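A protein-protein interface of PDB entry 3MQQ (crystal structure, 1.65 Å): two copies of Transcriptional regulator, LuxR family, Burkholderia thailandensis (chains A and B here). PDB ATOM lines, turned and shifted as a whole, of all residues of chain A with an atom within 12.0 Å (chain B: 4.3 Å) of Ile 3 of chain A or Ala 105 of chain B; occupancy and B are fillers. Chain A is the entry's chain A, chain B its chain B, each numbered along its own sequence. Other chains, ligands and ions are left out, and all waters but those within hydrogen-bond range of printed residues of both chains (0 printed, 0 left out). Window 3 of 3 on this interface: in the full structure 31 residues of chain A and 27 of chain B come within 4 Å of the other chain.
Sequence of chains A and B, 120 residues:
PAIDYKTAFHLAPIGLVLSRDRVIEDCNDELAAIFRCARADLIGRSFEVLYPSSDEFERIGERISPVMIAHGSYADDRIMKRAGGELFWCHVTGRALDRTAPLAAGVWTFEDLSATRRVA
Hydrophobic or aromatic side chains of chain A within 4 Å of the printed part of chain B: Ile 3, Ala 8 and Leu 11.
Hydrophobic or aromatic side chains of chain B within 4 Å of the printed part of chain A: Leu 18, Ala 105 and Val 107.
Along chain B the printed residues that touch a printed residue of chain A span positions 18 to 107.
Among the printed residues, no Asp or Glu carboxylate lies within 4 Å of a Lys or Arg side-chain nitrogen of the other chain.
The backbone carbonyl oxygen (O) of Gly 106 of chain B is in hydrogen-bond range of the backbone NH (N) of Ser 19 of chain B, at 2.9 Å.
N of Leu 97 of chain B is in hydrogen-bond range of O of Ala 105 of chain B (2.9 Å).
Among the printed residues, merely in contact across the chains: Ile 3 of chain A with Leu 18 of chain B, Ile 3 of chain A with Ala 105 of chain B, Ile 3 of chain A with Gly 106 of chain B, Ala 8 of chain A with Leu 18 of chain B, Ala 8 of chain A with Val 107 of chain B, Leu 11 of chain A with Ala 96 of chain B, Leu 11 of chain A with Leu 97 of chain B and Leu 11 of chain A with Val 107 of chain B.
Ile 3 of chain A touches just these residues of chain B: Leu 18 (3.4 Å), Ala 105 (3.7 Å) and Gly 106 (3.6 Å).
Printed residues of chain B within 4 Å of Ala 8 of chain A: Leu 18 (3.5 Å) and Val 107 (3.7 Å).
Printed residues of chain B within 4 Å of Leu 11 of chain A: Ala 96, Leu 97 and Val 107.
No residue of chain A comes within 4 Å of Ser 19 of chain B.
Of chain A, only Leu 11 comes within 4 Å of Ala 96 of chain B.
Ala 105 of chain B touches just one residue of chain A: Ile 3.
Of chain A, only Ile 3 (3.6 Å) comes within 4 Å of Gly 106 of chain B.
Of the printed residues of chain A, Val 107 of chain B touches Ala 8 and Leu 11.
The nearest printed residue of chain B that does not touch Ala 8 of chain A is Gly 106 of chain B (6.8 Å).
No position is printed for both chains.
Of the 8 pairs that touch across the chains among the printed residues, none has its exchanged pair printed and touching as well.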
ATOM      1  N   ILE A   3      11.287  20.755   4.527  1.00  0.00           N
ATOM      2  CA  ILE A   3      12.567  20.656   5.298  1.00  0.00           C
ATOM      3  C   ILE A   3      12.349  21.030   6.771  1.00  0.00           C
ATOM      4  O   ILE A   3      11.916  22.146   7.077  1.00  0.00           O
ATOM      5  CB  ILE A   3      13.674  21.539   4.659  1.00  0.00           C
ATOM      6  CG1 ILE A   3      14.074  20.983   3.287  1.00  0.00           C
ATOM      7  CG2 ILE A   3      14.896  21.635   5.568  1.00  0.00           C
ATOM      8  CD1 ILE A   3      14.874  21.955   2.437  1.00  0.00           C
ATOM      9  N   ASP A   4      12.608  20.083   7.677  1.00  0.00           N
ATOM     10  CA  ASP A   4      12.432  20.351   9.101  1.00  0.00           C
ATOM     11  C   ASP A   4      13.729  20.890   9.681  1.00  0.00           C
ATOM     12  O   ASP A   4      14.722  21.015   8.942  1.00  0.00           O
ATOM     13  CB  ASP A   4      11.842  19.153   9.880  1.00  0.00           C
ATOM     14  CG  ASP A   4      12.725  17.911   9.859  1.00  0.00           C
ATOM     15  OD1 ASP A   4      12.170  16.810  10.082  1.00  0.00           O
ATOM     16  OD2 ASP A   4      13.944  18.007   9.635  1.00  0.00           O
ATOM     17  N   TYR A   5      13.723  21.244  10.968  1.00  0.00           N
ATOM     18  CA  TYR A   5      14.851  22.001  11.525  1.00  0.00           C
ATOM     19  C   TYR A   5      16.111  21.137  11.643  1.00  0.00           C
ATOM     20  O   TYR A   5      17.234  21.653  11.468  1.00  0.00           O
ATOM     21  CB  TYR A   5      14.480  22.614  12.884  1.00  0.00           C
ATOM     22  CG  TYR A   5      13.378  23.653  12.822  1.00  0.00           C
ATOM     23  CD1 TYR A   5      13.598  24.866  12.184  1.00  0.00           C
ATOM     24  CD2 TYR A   5      12.128  23.433  13.416  1.00  0.00           C
ATOM     25  CE1 TYR A   5      12.619  25.823  12.108  1.00  0.00           C
ATOM     26  CE2 TYR A   5      11.126  24.415  13.353  1.00  0.00           C
ATOM     27  CZ  TYR A   5      11.401  25.611  12.699  1.00  0.00           C
ATOM     28  OH  TYR A   5      10.460  26.611  12.601  1.00  0.00           O
ATOM     29  N   LYS A   6      15.920  19.845  11.934  1.00  0.00           N
ATOM     30  CA  LYS A   6      17.030  18.875  11.985  1.00  0.00           C
ATOM     31  C   LYS A   6      17.720  18.720  10.628  1.00  0.00           C
ATOM     32  O   LYS A   6      18.944  18.822  10.537  1.00  0.00           O
ATOM     33  CB  LYS A   6      16.559  17.511  12.494  1.00  0.00           C
ATOM     34  CG  LYS A   6      17.700  16.532  12.710  1.00  0.00           C
ATOM     35  CD  LYS A   6      17.246  15.320  13.529  1.00  0.00           C
ATOM     36  CE  LYS A   6      18.400  14.353  13.774  1.00  0.00           C
ATOM     37  NZ  LYS A   6      18.056  13.307  14.788  1.00  0.00           N
ATOM     38  N   THR A   7      16.913  18.492   9.586  1.00  0.00           N
ATOM     39  CA  THR A   7      17.397  18.411   8.217  1.00  0.00           C
ATOM     40  C   THR A   7      18.144  19.682   7.788  1.00  0.00           C
ATOM     41  O   THR A   7      19.245  19.604   7.218  1.00  0.00           O
ATOM     42  CB  THR A   7      16.253  18.096   7.231  1.00  0.00           C
ATOM     43  OG1 THR A   7      15.661  16.834   7.574  1.00  0.00           O
ATOM     44  CG2 THR A   7      16.792  18.030   5.815  1.00  0.00           C
ATOM     45  N   ALA A   8      17.562  20.845   8.076  1.00  0.00           N
ATOM     46  CA  ALA A   8      18.213  22.125   7.782  1.00  0.00           C
ATOM     47  C   ALA A   8      19.613  22.214   8.390  1.00  0.00           C
ATOM     48  O   ALA A   8      20.558  22.609   7.708  1.00  0.00           O
ATOM     49  CB  ALA A   8      17.357  23.310   8.256  1.00  0.00           C
ATOM     50  N   PHE A   9      19.719  21.884   9.668  1.00  0.00           N
ATOM     51  CA  PHE A   9      21.002  21.922  10.382  1.00  0.00           C
ATOM     52  C   PHE A   9      22.000  21.052   9.632  1.00  0.00           C
ATOM     53  O   PHE A   9      23.106  21.495   9.335  1.00  0.00           O
ATOM     54  CB  PHE A   9      20.817  21.434  11.820  1.00  0.00           C
ATOM     55  CG  PHE A   9      22.085  21.387  12.623  1.00  0.00           C
ATOM     56  CD1 PHE A   9      22.467  22.474  13.385  1.00  0.00           C
ATOM     57  CD2 PHE A   9      22.844  20.217  12.700  1.00  0.00           C
ATOM     58  CE1 PHE A   9      23.628  22.462  14.131  1.00  0.00           C
ATOM     59  CE2 PHE A   9      24.006  20.168  13.484  1.00  0.00           C
ATOM     60  CZ  PHE A   9      24.396  21.291  14.220  1.00  0.00           C
ATOM     61  N   HIS A  10      21.576  19.839   9.289  1.00  0.00           N
ATOM     62  CA  HIS A  10      22.475  18.880   8.619  1.00  0.00           C
ATOM     63  C   HIS A  10      22.794  19.182   7.156  1.00  0.00           C
ATOM     64  O   HIS A  10      23.865  18.801   6.672  1.00  0.00           O
ATOM     65  CB  HIS A  10      21.992  17.447   8.799  1.00  0.00           C
ATOM     66  CG  HIS A  10      22.149  16.949  10.202  1.00  0.00           C
ATOM     67  ND1 HIS A  10      23.381  16.820  10.812  1.00  0.00           N
ATOM     68  CD2 HIS A  10      21.233  16.580  11.125  1.00  0.00           C
ATOM     69  CE1 HIS A  10      23.216  16.388  12.047  1.00  0.00           C
ATOM     70  NE2 HIS A  10      21.924  16.229  12.262  1.00  0.00           N
ATOM     71  N   LEU A  11      21.898  19.893   6.485  1.00  0.00           N
ATOM     72  CA  LEU A  11      22.052  20.267   5.067  1.00  0.00           C
ATOM     73  C   LEU A  11      22.834  21.570   4.849  1.00  0.00           C
ATOM     74  O   LEU A  11      23.282  21.838   3.725  1.00  0.00           O
ATOM     75  CB  LEU A  11      20.657  20.426   4.422  1.00  0.00           C
ATOM     76  CG  LEU A  11      20.448  20.678   2.911  1.00  0.00           C
ATOM     77  CD1 LEU A  11      21.005  19.519   2.099  1.00  0.00           C
ATOM     78  CD2 LEU A  11      18.977  20.921   2.554  1.00  0.00           C
ATOM     79  N   ALA A  12      22.963  22.383   5.900  1.00  0.00           N
ATOM     80  CA  ALA A  12      23.404  23.757   5.736  1.00  0.00           C
ATOM     81  C   ALA A  12      24.771  23.831   5.078  1.00  0.00           C
ATOM     82  O   ALA A  12      25.650  23.044   5.407  1.00  0.00           O
ATOM     83  CB  ALA A  12      23.413  24.501   7.076  1.00  0.00           C
ATOM     84  N   PRO A  13      24.947  24.795   4.163  1.00  0.00           N
ATOM     85  CA  PRO A  13      26.186  24.987   3.410  1.00  0.00           C
ATOM     86  C   PRO A  13      27.316  25.649   4.189  1.00  0.00           C
ATOM     87  O   PRO A  13      28.367  25.940   3.615  1.00  0.00           O
ATOM     88  CB  PRO A  13      25.749  25.890   2.247  1.00  0.00           C
ATOM     89  CG  PRO A  13      24.597  26.629   2.783  1.00  0.00           C
ATOM     90  CD  PRO A  13      23.873  25.673   3.669  1.00  0.00           C
ATOM     91  N   LEU A  16      28.046  24.283  11.179  1.00  0.00           N
ATOM     92  CA  LEU A  16      27.203  24.700  12.293  1.00  0.00           C
ATOM     93  C   LEU A  16      27.563  23.850  13.504  1.00  0.00           C
ATOM     94  O   LEU A  16      27.863  22.645  13.369  1.00  0.00           O
ATOM     95  CB  LEU A  16      25.733  24.516  11.974  1.00  0.00           C
ATOM     96  CG  LEU A  16      25.138  25.355  10.859  1.00  0.00           C
ATOM     97  CD1 LEU A  16      23.711  24.866  10.687  1.00  0.00           C
ATOM     98  CD2 LEU A  16      25.178  26.855  11.235  1.00  0.00           C
ATOM     99  N   ASN A  28      27.357  19.716  12.000  1.00  0.00           N
ATOM    100  CA  ASN A  28      26.872  19.203  10.719  1.00  0.00           C
ATOM    101  C   ASN A  28      28.039  18.723   9.872  1.00  0.00           C
ATOM    102  O   ASN A  28      29.208  18.924  10.241  1.00  0.00           O
ATOM    103  CB  ASN A  28      25.975  20.229  10.002  1.00  0.00           C
ATOM    104  CG  ASN A  28      26.726  21.501   9.613  1.00  0.00           C
ATOM    105  OD1 ASN A  28      27.926  21.654   9.880  1.00  0.00           O
ATOM    106  ND2 ASN A  28      26.012  22.422   8.984  1.00  0.00           N
ATOM    107  N   LEU B  18      14.323  28.560   5.380  1.00  0.00           N
ATOM    108  CA  LEU B  18      13.922  27.304   4.729  1.00  0.00           C
ATOM    109  C   LEU B  18      13.057  27.703   3.533  1.00  0.00           C
ATOM    110  O   LEU B  18      12.049  28.364   3.717  1.00  0.00           O
ATOM    111  CB  LEU B  18      13.148  26.396   5.704  1.00  0.00           C
ATOM    112  CG  LEU B  18      13.774  26.255   7.083  1.00  0.00           C
ATOM    113  CD1 LEU B  18      12.921  25.311   7.982  1.00  0.00           C
ATOM    114  CD2 LEU B  18      15.210  25.723   6.934  1.00  0.00           C
ATOM    115  N   SER B  19      13.521  27.400   2.317  1.00  0.00           N
ATOM    116  CA  SER B  19      12.853  27.900   1.097  1.00  0.00           C
ATOM    117  C   SER B  19      12.186  26.762   0.333  1.00  0.00           C
ATOM    118  O   SER B  19      12.392  25.555   0.607  1.00  0.00           O
ATOM    119  CB  SER B  19      13.864  28.597   0.190  1.00  0.00           C
ATOM    120  OG  SER B  19      14.718  27.612  -0.421  1.00  0.00           O
ATOM    121  N   ARG B  20      11.346  27.170  -0.614  1.00  0.00           N
ATOM    122  CA  ARG B  20      10.790  26.247  -1.616  1.00  0.00           C
ATOM    123  C   ARG B  20      10.396  27.103  -2.806  1.00  0.00           C
ATOM    124  O   ARG B  20       9.665  28.084  -2.649  1.00  0.00           O
ATOM    125  CB  ARG B  20       9.606  25.456  -1.052  1.00  0.00           C
ATOM    126  CG  ARG B  20       9.055  24.437  -2.002  1.00  0.00           C
ATOM    127  CD  ARG B  20       8.401  23.285  -1.234  1.00  0.00           C
ATOM    128  NE  ARG B  20       7.145  23.610  -0.545  1.00  0.00           N
ATOM    129  CZ  ARG B  20       6.268  24.558  -0.891  1.00  0.00           C
ATOM    130  NH1 ARG B  20       5.163  24.711  -0.177  1.00  0.00           N
ATOM    131  NH2 ARG B  20       6.483  25.366  -1.922  1.00  0.00           N
ATOM    132  N   ALA B  96      20.640  23.294  -1.857  1.00  0.00           N
ATOM    133  CA  ALA B  96      19.372  22.678  -2.263  1.00  0.00           C
ATOM    134  C   ALA B  96      19.281  21.283  -1.680  1.00  0.00           C
ATOM    135  O   ALA B  96      20.287  20.572  -1.579  1.00  0.00           O
ATOM    136  CB  ALA B  96      19.281  22.617  -3.784  1.00  0.00           C
ATOM    137  N   LEU B  97      18.067  20.876  -1.337  1.00  0.00           N
ATOM    138  CA  LEU B  97      17.804  19.535  -0.873  1.00  0.00           C
ATOM    139  C   LEU B  97      18.168  18.498  -1.952  1.00  0.00           C
ATOM    140  O   LEU B  97      18.636  17.402  -1.632  1.00  0.00           O
ATOM    141  CB  LEU B  97      16.340  19.409  -0.440  1.00  0.00           C
ATOM    142  CG  LEU B  97      15.917  18.086   0.205  1.00  0.00           C
ATOM    143  CD1 LEU B  97      16.605  17.813   1.560  1.00  0.00           C
ATOM    144  CD2 LEU B  97      14.392  18.020   0.325  1.00  0.00           C
ATOM    145  N   ALA B 104      14.541  24.737  -5.913  1.00  0.00           N
ATOM    146  CA  ALA B 104      13.426  24.148  -5.154  1.00  0.00           C
ATOM    147  C   ALA B 104      13.696  24.202  -3.633  1.00  0.00           C
ATOM    148  O   ALA B 104      14.274  25.182  -3.141  1.00  0.00           O
ATOM    149  CB  ALA B 104      13.141  22.695  -5.647  1.00  0.00           C
ATOM    150  N   ALA B 105      13.275  23.199  -2.862  1.00  0.00           N
ATOM    151  CA  ALA B 105      13.502  23.276  -1.417  1.00  0.00           C
ATOM    152  C   ALA B 105      14.995  23.428  -1.107  1.00  0.00           C
ATOM    153  O   ALA B 105      15.835  22.763  -1.706  1.00  0.00           O
ATOM    154  CB  ALA B 105      12.928  22.057  -0.696  1.00  0.00           C
ATOM    155  N   GLY B 106      15.323  24.329  -0.187  1.00  0.00           N
ATOM    156  CA  GLY B 106      16.698  24.402   0.276  1.00  0.00           C
ATOM    157  C   GLY B 106      16.839  25.201   1.552  1.00  0.00           C
ATOM    158  O   GLY B 106      15.862  25.728   2.082  1.00  0.00           O
ATOM    159  N   VAL B 107      18.075  25.232   2.048  1.00  0.00           N
ATOM    160  CA  VAL B 107      18.434  26.048   3.219  1.00  0.00           C
ATOM    161  C   VAL B 107      19.343  27.175   2.731  1.00  0.00           C
ATOM    162  O   VAL B 107      20.329  26.938   2.054  1.00  0.00           O
ATOM    163  CB  VAL B 107      19.120  25.195   4.343  1.00  0.00           C
ATOM    164  CG1 VAL B 107      19.258  25.984   5.674  1.00  0.00           C
ATOM    165  CG2 VAL B 107      18.320  23.944   4.618  1.00  0.00           C
